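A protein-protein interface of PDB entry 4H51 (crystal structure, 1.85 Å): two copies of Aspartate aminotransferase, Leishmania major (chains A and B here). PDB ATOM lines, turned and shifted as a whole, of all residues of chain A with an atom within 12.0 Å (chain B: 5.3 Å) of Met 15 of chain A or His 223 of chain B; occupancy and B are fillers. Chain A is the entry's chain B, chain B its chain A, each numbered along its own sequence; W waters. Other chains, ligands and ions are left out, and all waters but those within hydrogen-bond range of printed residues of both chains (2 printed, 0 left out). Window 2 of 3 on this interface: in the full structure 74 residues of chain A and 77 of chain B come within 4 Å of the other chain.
OE1 of Gln 225 of chain B sits at hydrogen-bond distance from NE1 of Trp 21 of chain A, 2.9 Å away.
The backbone NH (N) of Gly 190 of chain B sits at hydrogen-bond distance from the backbone carbonyl oxygen (O) of Lys 222 of chain B.
The backbone NH (N) of Gly 190 of chain B lies close to the backbone carbonyl oxygen (O) of His 223 of chain B.
N of Ser 191 of chain B sits at hydrogen-bond distance from ND1 of His 224 of chain B.
The backbone carbonyl oxygen (O) of Ser 191 of chain B is in hydrogen-bond range of the backbone NH (N) of Gln 225 of chain B (2.8 Å).
The backbone carbonyl oxygen of Met 219 of chain B lies within hydrogen-bond range of the backbone NH of His 224 of chain B, 3.0 Å away.
Met 15 of chain A touches His 223 of chain B (O to CB, 3.4 Å).
Thr 17 of chain A touches His 223 of chain B.
Thr 17 of chain A touches His 224 of chain B (CG2 to O, 3.2 Å).
CG2 of Thr 17 of chain A touches N of Gln 225 of chain B, 3.97 Å away.
Arg 20 of chain A touches Gly 190 of chain B.
Met 15 of chain A touches just one residue of chain B: His 223 (3.4 Å).
No residue of chain A comes within 4 Å of Asp 189 of chain B.
Gly 190 of chain B touches just one residue of chain A: Arg 20 (3.7 Å).
No residue of chain A comes within 4 Å of Ser 191 of chain B.
No residue of chain A comes within 4 Å of Ala 221 of chain B.
No residue of chain A comes within 4 Å of Lys 222 of chain B.
Printed residues of chain A within 4 Å of His 224 of chain B: Thr 17 (3.2 Å).
Of the printed residues of chain B, Thr 17 of chain A touches His 223 (3.6 Å), His 224 (3.2 Å) and Gln 225 (3.97 Å).
Of the printed residues of chain B, Arg 20 of chain A touches Gly 190.
Of the printed residues of chain A, Gln 225 of chain B touches Thr 17 (3.97 Å) and Trp 21 (2.9 Å).
Of the printed residues of chain B, Trp 21 of chain A touches Gln 225.
The nearest printed residue of chain B that does not touch Met 15 of chain A is Gly 190 of chain B (5.7 Å).
The nearest residue of chain A that does not touch His 223 of chain B is Thr 16 of chain A (4.3 Å).
Hydrophobic or aromatic side chains of chain B that line the printed part of chain A: His 223.
Of the 10 printed residues of chain A, 4 touch a printed residue of chain B.
Printed residues of chain A that touch a printed residue of chain B: Met 15, Thr 17, Arg 20 and Trp 21.
Hydrophobic or aromatic side chains of chain A within 4 Å of the printed part of chain B: Trp 21.
Among the printed residues, 6 pairs touch across the chains.
No position is printed for both chains.
Of the 6 pairs that touch across the chains among the printed residues, none has its exchanged pair printed and touching as well.
Water W2 lies within hydrogen-bond range of NE of Arg 20 of chain A, O of Met 15 of chain A, O of His 223 of chain B and N of Thr 17 of chain A.
Water W1 bridges the backbone carbonyl oxygen (O) of Gly 190 of chain B (2.7 Å) and the guanidinium group (NH2) of Arg 20 of chain A (3.4 Å).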
ATOM      1  N   MET A  15     -13.411  -1.802 -11.339  1.00  0.00           N
ATOM      2  CA  MET A  15     -12.036  -2.285 -11.731  1.00  0.00           C
ATOM      3  C   MET A  15     -12.041  -3.716 -12.291  1.00  0.00           C
ATOM      4  O   MET A  15     -12.386  -4.653 -11.579  1.00  0.00           O
ATOM      5  CB  MET A  15     -11.073  -2.192 -10.553  1.00  0.00           C
ATOM      6  CG  MET A  15      -9.610  -2.327 -10.957  1.00  0.00           C
ATOM      7  SD  MET A  15      -8.392  -2.012  -9.662  1.00  0.00           S
ATOM      8  CE  MET A  15      -8.525  -0.210  -9.507  1.00  0.00           C
ATOM      9  N   THR A  16     -11.633  -3.868 -13.551  1.00  0.00           N
ATOM     10  CA  THR A  16     -11.572  -5.162 -14.237  1.00  0.00           C
ATOM     11  C   THR A  16     -10.369  -5.969 -13.776  1.00  0.00           C
ATOM     12  O   THR A  16      -9.418  -5.413 -13.208  1.00  0.00           O
ATOM     13  CB  THR A  16     -11.464  -4.979 -15.765  1.00  0.00           C
ATOM     14  OG1 THR A  16     -10.187  -4.406 -16.084  1.00  0.00           O
ATOM     15  CG2 THR A  16     -12.597  -4.036 -16.299  1.00  0.00           C
ATOM     16  N   THR A  17     -10.378  -7.276 -14.016  1.00  0.00           N
ATOM     17  CA  THR A  17      -9.221  -8.062 -13.661  1.00  0.00           C
ATOM     18  C   THR A  17      -8.014  -7.614 -14.490  1.00  0.00           C
ATOM     19  O   THR A  17      -6.901  -7.569 -13.977  1.00  0.00           O
ATOM     20  CB  THR A  17      -9.419  -9.594 -13.795  1.00  0.00           C
ATOM     21  OG1 THR A  17      -9.722  -9.932 -15.140  1.00  0.00           O
ATOM     22  CG2 THR A  17     -10.528 -10.064 -12.856  1.00  0.00           C
ATOM     23  N   ALA A  18      -8.241  -7.234 -15.745  1.00  0.00           N
ATOM     24  CA  ALA A  18      -7.125  -6.753 -16.559  1.00  0.00           C
ATOM     25  C   ALA A  18      -6.445  -5.548 -15.866  1.00  0.00           C
ATOM     26  O   ALA A  18      -5.228  -5.475 -15.795  1.00  0.00           O
ATOM     27  CB  ALA A  18      -7.576  -6.417 -17.965  1.00  0.00           C
ATOM     28  N   GLU A  19      -7.249  -4.630 -15.333  1.00  0.00           N
ATOM     29  CA  GLU A  19      -6.725  -3.439 -14.630  1.00  0.00           C
ATOM     30  C   GLU A  19      -6.024  -3.786 -13.323  1.00  0.00           C
ATOM     31  O   GLU A  19      -5.028  -3.169 -12.976  1.00  0.00           O
ATOM     32  CB  GLU A  19      -7.871  -2.440 -14.389  1.00  0.00           C
ATOM     33  CG  GLU A  19      -8.397  -1.819 -15.697  1.00  0.00           C
ATOM     34  CD  GLU A  19      -9.797  -1.225 -15.593  1.00  0.00           C
ATOM     35  OE1 GLU A  19     -10.173  -0.457 -16.498  1.00  0.00           O
ATOM     36  OE2 GLU A  19     -10.550  -1.528 -14.638  1.00  0.00           O
ATOM     37  N   ARG A  20      -6.483  -4.816 -12.616  1.00  0.00           N
ATOM     38  CA  ARG A  20      -5.802  -5.234 -11.392  1.00  0.00           C
ATOM     39  C   ARG A  20      -4.430  -5.873 -11.646  1.00  0.00           C
ATOM     40  O   ARG A  20      -3.504  -5.649 -10.858  1.00  0.00           O
ATOM     41  CB  ARG A  20      -6.608  -6.247 -10.590  1.00  0.00           C
ATOM     42  CG  ARG A  20      -7.898  -5.732  -9.973  1.00  0.00           C
ATOM     43  CD  ARG A  20      -8.455  -6.729  -8.939  1.00  0.00           C
ATOM     44  NE  ARG A  20      -9.828  -6.381  -8.577  1.00  0.00           N
ATOM     45  CZ  ARG A  20     -10.175  -5.587  -7.568  1.00  0.00           C
ATOM     46  NH1 ARG A  20      -9.266  -5.059  -6.753  1.00  0.00           N
ATOM     47  NH2 ARG A  20     -11.449  -5.353  -7.343  1.00  0.00           N
ATOM     48  N   TRP A  21      -4.316  -6.705 -12.685  1.00  0.00           N
ATOM     49  CA  TRP A  21      -3.036  -7.292 -13.044  1.00  0.00           C
ATOM     50  C   TRP A  21      -2.051  -6.238 -13.491  1.00  0.00           C
ATOM     51  O   TRP A  21      -0.849  -6.380 -13.296  1.00  0.00           O
ATOM     52  CB  TRP A  21      -3.154  -8.382 -14.127  1.00  0.00           C
ATOM     53  CG  TRP A  21      -3.678  -9.698 -13.566  1.00  0.00           C
ATOM     54  CD1 TRP A  21      -5.000 -10.161 -13.598  1.00  0.00           C
ATOM     55  CD2 TRP A  21      -2.924 -10.743 -12.862  1.00  0.00           C
ATOM     56  NE1 TRP A  21      -5.104 -11.372 -12.961  1.00  0.00           N
ATOM     57  CE2 TRP A  21      -3.900 -11.787 -12.507  1.00  0.00           C
ATOM     58  CE3 TRP A  21      -1.585 -10.918 -12.491  1.00  0.00           C
ATOM     59  CZ2 TRP A  21      -3.532 -12.933 -11.840  1.00  0.00           C
ATOM     60  CZ3 TRP A  21      -1.234 -12.070 -11.805  1.00  0.00           C
ATOM     61  CH2 TRP A  21      -2.176 -13.060 -11.485  1.00  0.00           C
ATOM     62  N   GLN A  22      -2.559  -5.197 -14.137  1.00  0.00           N
ATOM     63  CA  GLN A  22      -1.736  -4.056 -14.539  1.00  0.00           C
ATOM     64  C   GLN A  22      -0.894  -3.538 -13.365  1.00  0.00           C
ATOM     65  O   GLN A  22       0.238  -3.112 -13.550  1.00  0.00           O
ATOM     66  CB  GLN A  22      -2.621  -2.940 -15.157  1.00  0.00           C
ATOM     67  CG  GLN A  22      -1.881  -1.958 -16.061  1.00  0.00           C
ATOM     68  CD  GLN A  22      -1.405  -2.578 -17.376  1.00  0.00           C
ATOM     69  OE1 GLN A  22      -2.127  -3.317 -18.038  1.00  0.00           O
ATOM     70  NE2 GLN A  22      -0.181  -2.252 -17.769  1.00  0.00           N
ATOM     71  N   LYS A  23      -1.422  -3.609 -12.153  1.00  0.00           N
ATOM     72  CA  LYS A  23      -0.765  -3.046 -10.991  1.00  0.00           C
ATOM     73  C   LYS A  23       0.355  -3.923 -10.383  1.00  0.00           C
ATOM     74  O   LYS A  23       1.084  -3.472  -9.493  1.00  0.00           O
ATOM     75  CB  LYS A  23      -1.835  -2.696  -9.941  1.00  0.00           C
ATOM     76  N   ILE A  24       0.524  -5.162 -10.857  1.00  0.00           N
ATOM     77  CA  ILE A  24       1.563  -6.037 -10.290  1.00  0.00           C
ATOM     78  C   ILE A  24       2.969  -5.441 -10.550  1.00  0.00           C
ATOM     79  O   ILE A  24       3.245  -4.926 -11.633  1.00  0.00           O
ATOM     80  CB  ILE A  24       1.461  -7.488 -10.841  1.00  0.00           C
ATOM     81  CG1 ILE A  24       1.922  -8.497  -9.775  1.00  0.00           C
ATOM     82  CG2 ILE A  24       2.204  -7.617 -12.165  1.00  0.00           C
ATOM     83  CD1 ILE A  24       1.863  -9.931 -10.221  1.00  0.00           C
ATOM     84  N   ASP B 189     -17.713  -7.522  -5.797  1.00  0.00           N
ATOM     85  CA  ASP B 189     -16.962  -7.452  -7.049  1.00  0.00           C
ATOM     86  C   ASP B 189     -15.463  -7.712  -6.773  1.00  0.00           C
ATOM     87  O   ASP B 189     -14.913  -7.294  -5.737  1.00  0.00           O
ATOM     88  CB  ASP B 189     -17.155  -6.075  -7.731  1.00  0.00           C
ATOM     89  CG  ASP B 189     -18.532  -5.912  -8.434  1.00  0.00           C
ATOM     90  OD1 ASP B 189     -19.437  -6.753  -8.288  1.00  0.00           O
ATOM     91  OD2 ASP B 189     -18.721  -4.903  -9.137  1.00  0.00           O
ATOM     92  N   GLY B 190     -14.787  -8.370  -7.689  1.00  0.00           N
ATOM     93  CA  GLY B 190     -13.339  -8.571  -7.536  1.00  0.00           C
ATOM     94  C   GLY B 190     -12.927  -9.588  -6.477  1.00  0.00           C
ATOM     95  O   GLY B 190     -11.937  -9.402  -5.744  1.00  0.00           O
ATOM     96  N   SER B 191     -13.704 -10.655  -6.375  1.00  0.00           N
ATOM     97  CA  SER B 191     -13.359 -11.804  -5.555  1.00  0.00           C
ATOM     98  C   SER B 191     -12.633 -12.830  -6.420  1.00  0.00           C
ATOM     99  O   SER B 191     -12.568 -12.690  -7.643  1.00  0.00           O
ATOM    100  CB  SER B 191     -14.627 -12.380  -4.939  1.00  0.00           C
ATOM    101  OG  SER B 191     -15.291 -11.368  -4.163  1.00  0.00           O
ATOM    102  N   LEU B 218     -21.173 -14.251 -15.674  1.00  0.00           N
ATOM    103  CA  LEU B 218     -21.166 -13.767 -14.282  1.00  0.00           C
ATOM    104  C   LEU B 218     -19.769 -13.331 -13.825  1.00  0.00           C
ATOM    105  O   LEU B 218     -19.587 -12.237 -13.261  1.00  0.00           O
ATOM    106  CB  LEU B 218     -21.738 -14.815 -13.339  1.00  0.00           C
ATOM    107  CG  LEU B 218     -23.218 -15.103 -13.558  1.00  0.00           C
ATOM    108  CD1 LEU B 218     -23.718 -16.223 -12.654  1.00  0.00           C
ATOM    109  CD2 LEU B 218     -23.994 -13.840 -13.316  1.00  0.00           C
ATOM    110  N   MET B 219     -18.757 -14.155 -14.073  1.00  0.00           N
ATOM    111  CA  MET B 219     -17.409 -13.774 -13.642  1.00  0.00           C
ATOM    112  C   MET B 219     -16.972 -12.448 -14.293  1.00  0.00           C
ATOM    113  O   MET B 219     -16.371 -11.569 -13.636  1.00  0.00           O
ATOM    114  CB  MET B 219     -16.402 -14.863 -13.961  1.00  0.00           C
ATOM    115  CG  MET B 219     -16.671 -16.161 -13.243  1.00  0.00           C
ATOM    116  SD  MET B 219     -16.366 -16.034 -11.480  1.00  0.00           S
ATOM    117  CE  MET B 219     -17.184 -17.543 -10.961  1.00  0.00           C
ATOM    118  N   LEU B 220     -17.297 -12.274 -15.566  1.00  0.00           N
ATOM    119  CA  LEU B 220     -16.989 -11.011 -16.224  1.00  0.00           C
ATOM    120  C   LEU B 220     -17.776  -9.868 -15.625  1.00  0.00           C
ATOM    121  O   LEU B 220     -17.214  -8.813 -15.349  1.00  0.00           O
ATOM    122  CB  LEU B 220     -17.293 -11.097 -17.714  1.00  0.00           C
ATOM    123  CG  LEU B 220     -16.196 -11.750 -18.529  1.00  0.00           C
ATOM    124  CD1 LEU B 220     -16.707 -12.008 -19.915  1.00  0.00           C
ATOM    125  CD2 LEU B 220     -14.928 -10.893 -18.507  1.00  0.00           C
ATOM    126  N   ALA B 221     -19.082 -10.071 -15.430  1.00  0.00           N
ATOM    127  CA  ALA B 221     -19.941  -8.980 -14.969  1.00  0.00           C
ATOM    128  C   ALA B 221     -19.540  -8.474 -13.592  1.00  0.00           C
ATOM    129  O   ALA B 221     -19.700  -7.287 -13.328  1.00  0.00           O
ATOM    130  CB  ALA B 221     -21.407  -9.386 -14.970  1.00  0.00           C
ATOM    131  N   LYS B 222     -19.028  -9.374 -12.747  1.00  0.00           N
ATOM    132  CA  LYS B 222     -18.679  -9.115 -11.350  1.00  0.00           C
ATOM    133  C   LYS B 222     -17.160  -8.797 -11.164  1.00  0.00           C
ATOM    134  O   LYS B 222     -16.704  -8.464 -10.063  1.00  0.00           O
ATOM    135  CB  LYS B 222     -19.035 -10.356 -10.505  1.00  0.00           C
ATOM    136  CG  LYS B 222     -20.519 -10.549 -10.194  1.00  0.00           C
ATOM    137  CD  LYS B 222     -21.118  -9.478  -9.299  1.00  0.00           C
ATOM    138  CE  LYS B 222     -20.628  -9.551  -7.862  1.00  0.00           C
ATOM    139  NZ  LYS B 222     -21.143  -8.429  -7.036  1.00  0.00           N
ATOM    140  N   HIS B 223     -16.401  -8.870 -12.257  1.00  0.00           N
ATOM    141  CA  HIS B 223     -14.976  -8.594 -12.276  1.00  0.00           C
ATOM    142  C   HIS B 223     -14.221  -9.527 -11.353  1.00  0.00           C
ATOM    143  O   HIS B 223     -13.229  -9.139 -10.721  1.00  0.00           O
ATOM    144  CB  HIS B 223     -14.702  -7.122 -11.943  1.00  0.00           C
ATOM    145  CG  HIS B 223     -15.694  -6.153 -12.565  1.00  0.00           C
ATOM    146  ND1 HIS B 223     -15.752  -5.918 -13.893  1.00  0.00           N
ATOM    147  CD2 HIS B 223     -16.684  -5.370 -11.990  1.00  0.00           C
ATOM    148  CE1 HIS B 223     -16.718  -5.034 -14.156  1.00  0.00           C
ATOM    149  NE2 HIS B 223     -17.294  -4.691 -12.993  1.00  0.00           N
ATOM    150  N   HIS B 224     -14.658 -10.788 -11.295  1.00  0.00           N
ATOM    151  CA  HIS B 224     -14.014 -11.805 -10.442  1.00  0.00           C
ATOM    152  C   HIS B 224     -12.791 -12.376 -11.110  1.00  0.00           C
ATOM    153  O   HIS B 224     -12.709 -12.406 -12.334  1.00  0.00           O
ATOM    154  CB  HIS B 224     -14.971 -12.964 -10.164  1.00  0.00           C
ATOM    155  CG  HIS B 224     -16.112 -12.613  -9.253  1.00  0.00           C
ATOM    156  ND1 HIS B 224     -15.988 -11.763  -8.214  1.00  0.00           N
ATOM    157  CD2 HIS B 224     -17.401 -13.091  -9.211  1.00  0.00           C
ATOM    158  CE1 HIS B 224     -17.174 -11.667  -7.587  1.00  0.00           C
ATOM    159  NE2 HIS B 224     -18.032 -12.475  -8.194  1.00  0.00           N
ATOM    160  N   GLN B 225     -11.835 -12.829 -10.317  1.00  0.00           N
ATOM    161  CA  GLN B 225     -10.677 -13.575 -10.806  1.00  0.00           C
ATOM    162  C   GLN B 225     -11.036 -15.032 -10.844  1.00  0.00           C
ATOM    163  O   GLN B 225     -11.519 -15.605  -9.839  1.00  0.00           O
ATOM    164  CB  GLN B 225      -9.457 -13.404  -9.884  1.00  0.00           C
ATOM    165  CG  GLN B 225      -8.278 -14.274 -10.267  1.00  0.00           C
ATOM    166  CD  GLN B 225      -7.625 -13.859 -11.584  1.00  0.00           C
ATOM    167  OE1 GLN B 225      -7.416 -12.661 -11.827  1.00  0.00           O
ATOM    168  NE2 GLN B 225      -7.315 -14.819 -12.426  1.00  0.00           N
HETATM  169  O   HOH W   1     -10.842  -7.220  -4.531  1.00  0.00           O
HETATM  170  O   HOH W   2     -11.323  -7.081 -10.698  1.00  0.00           O
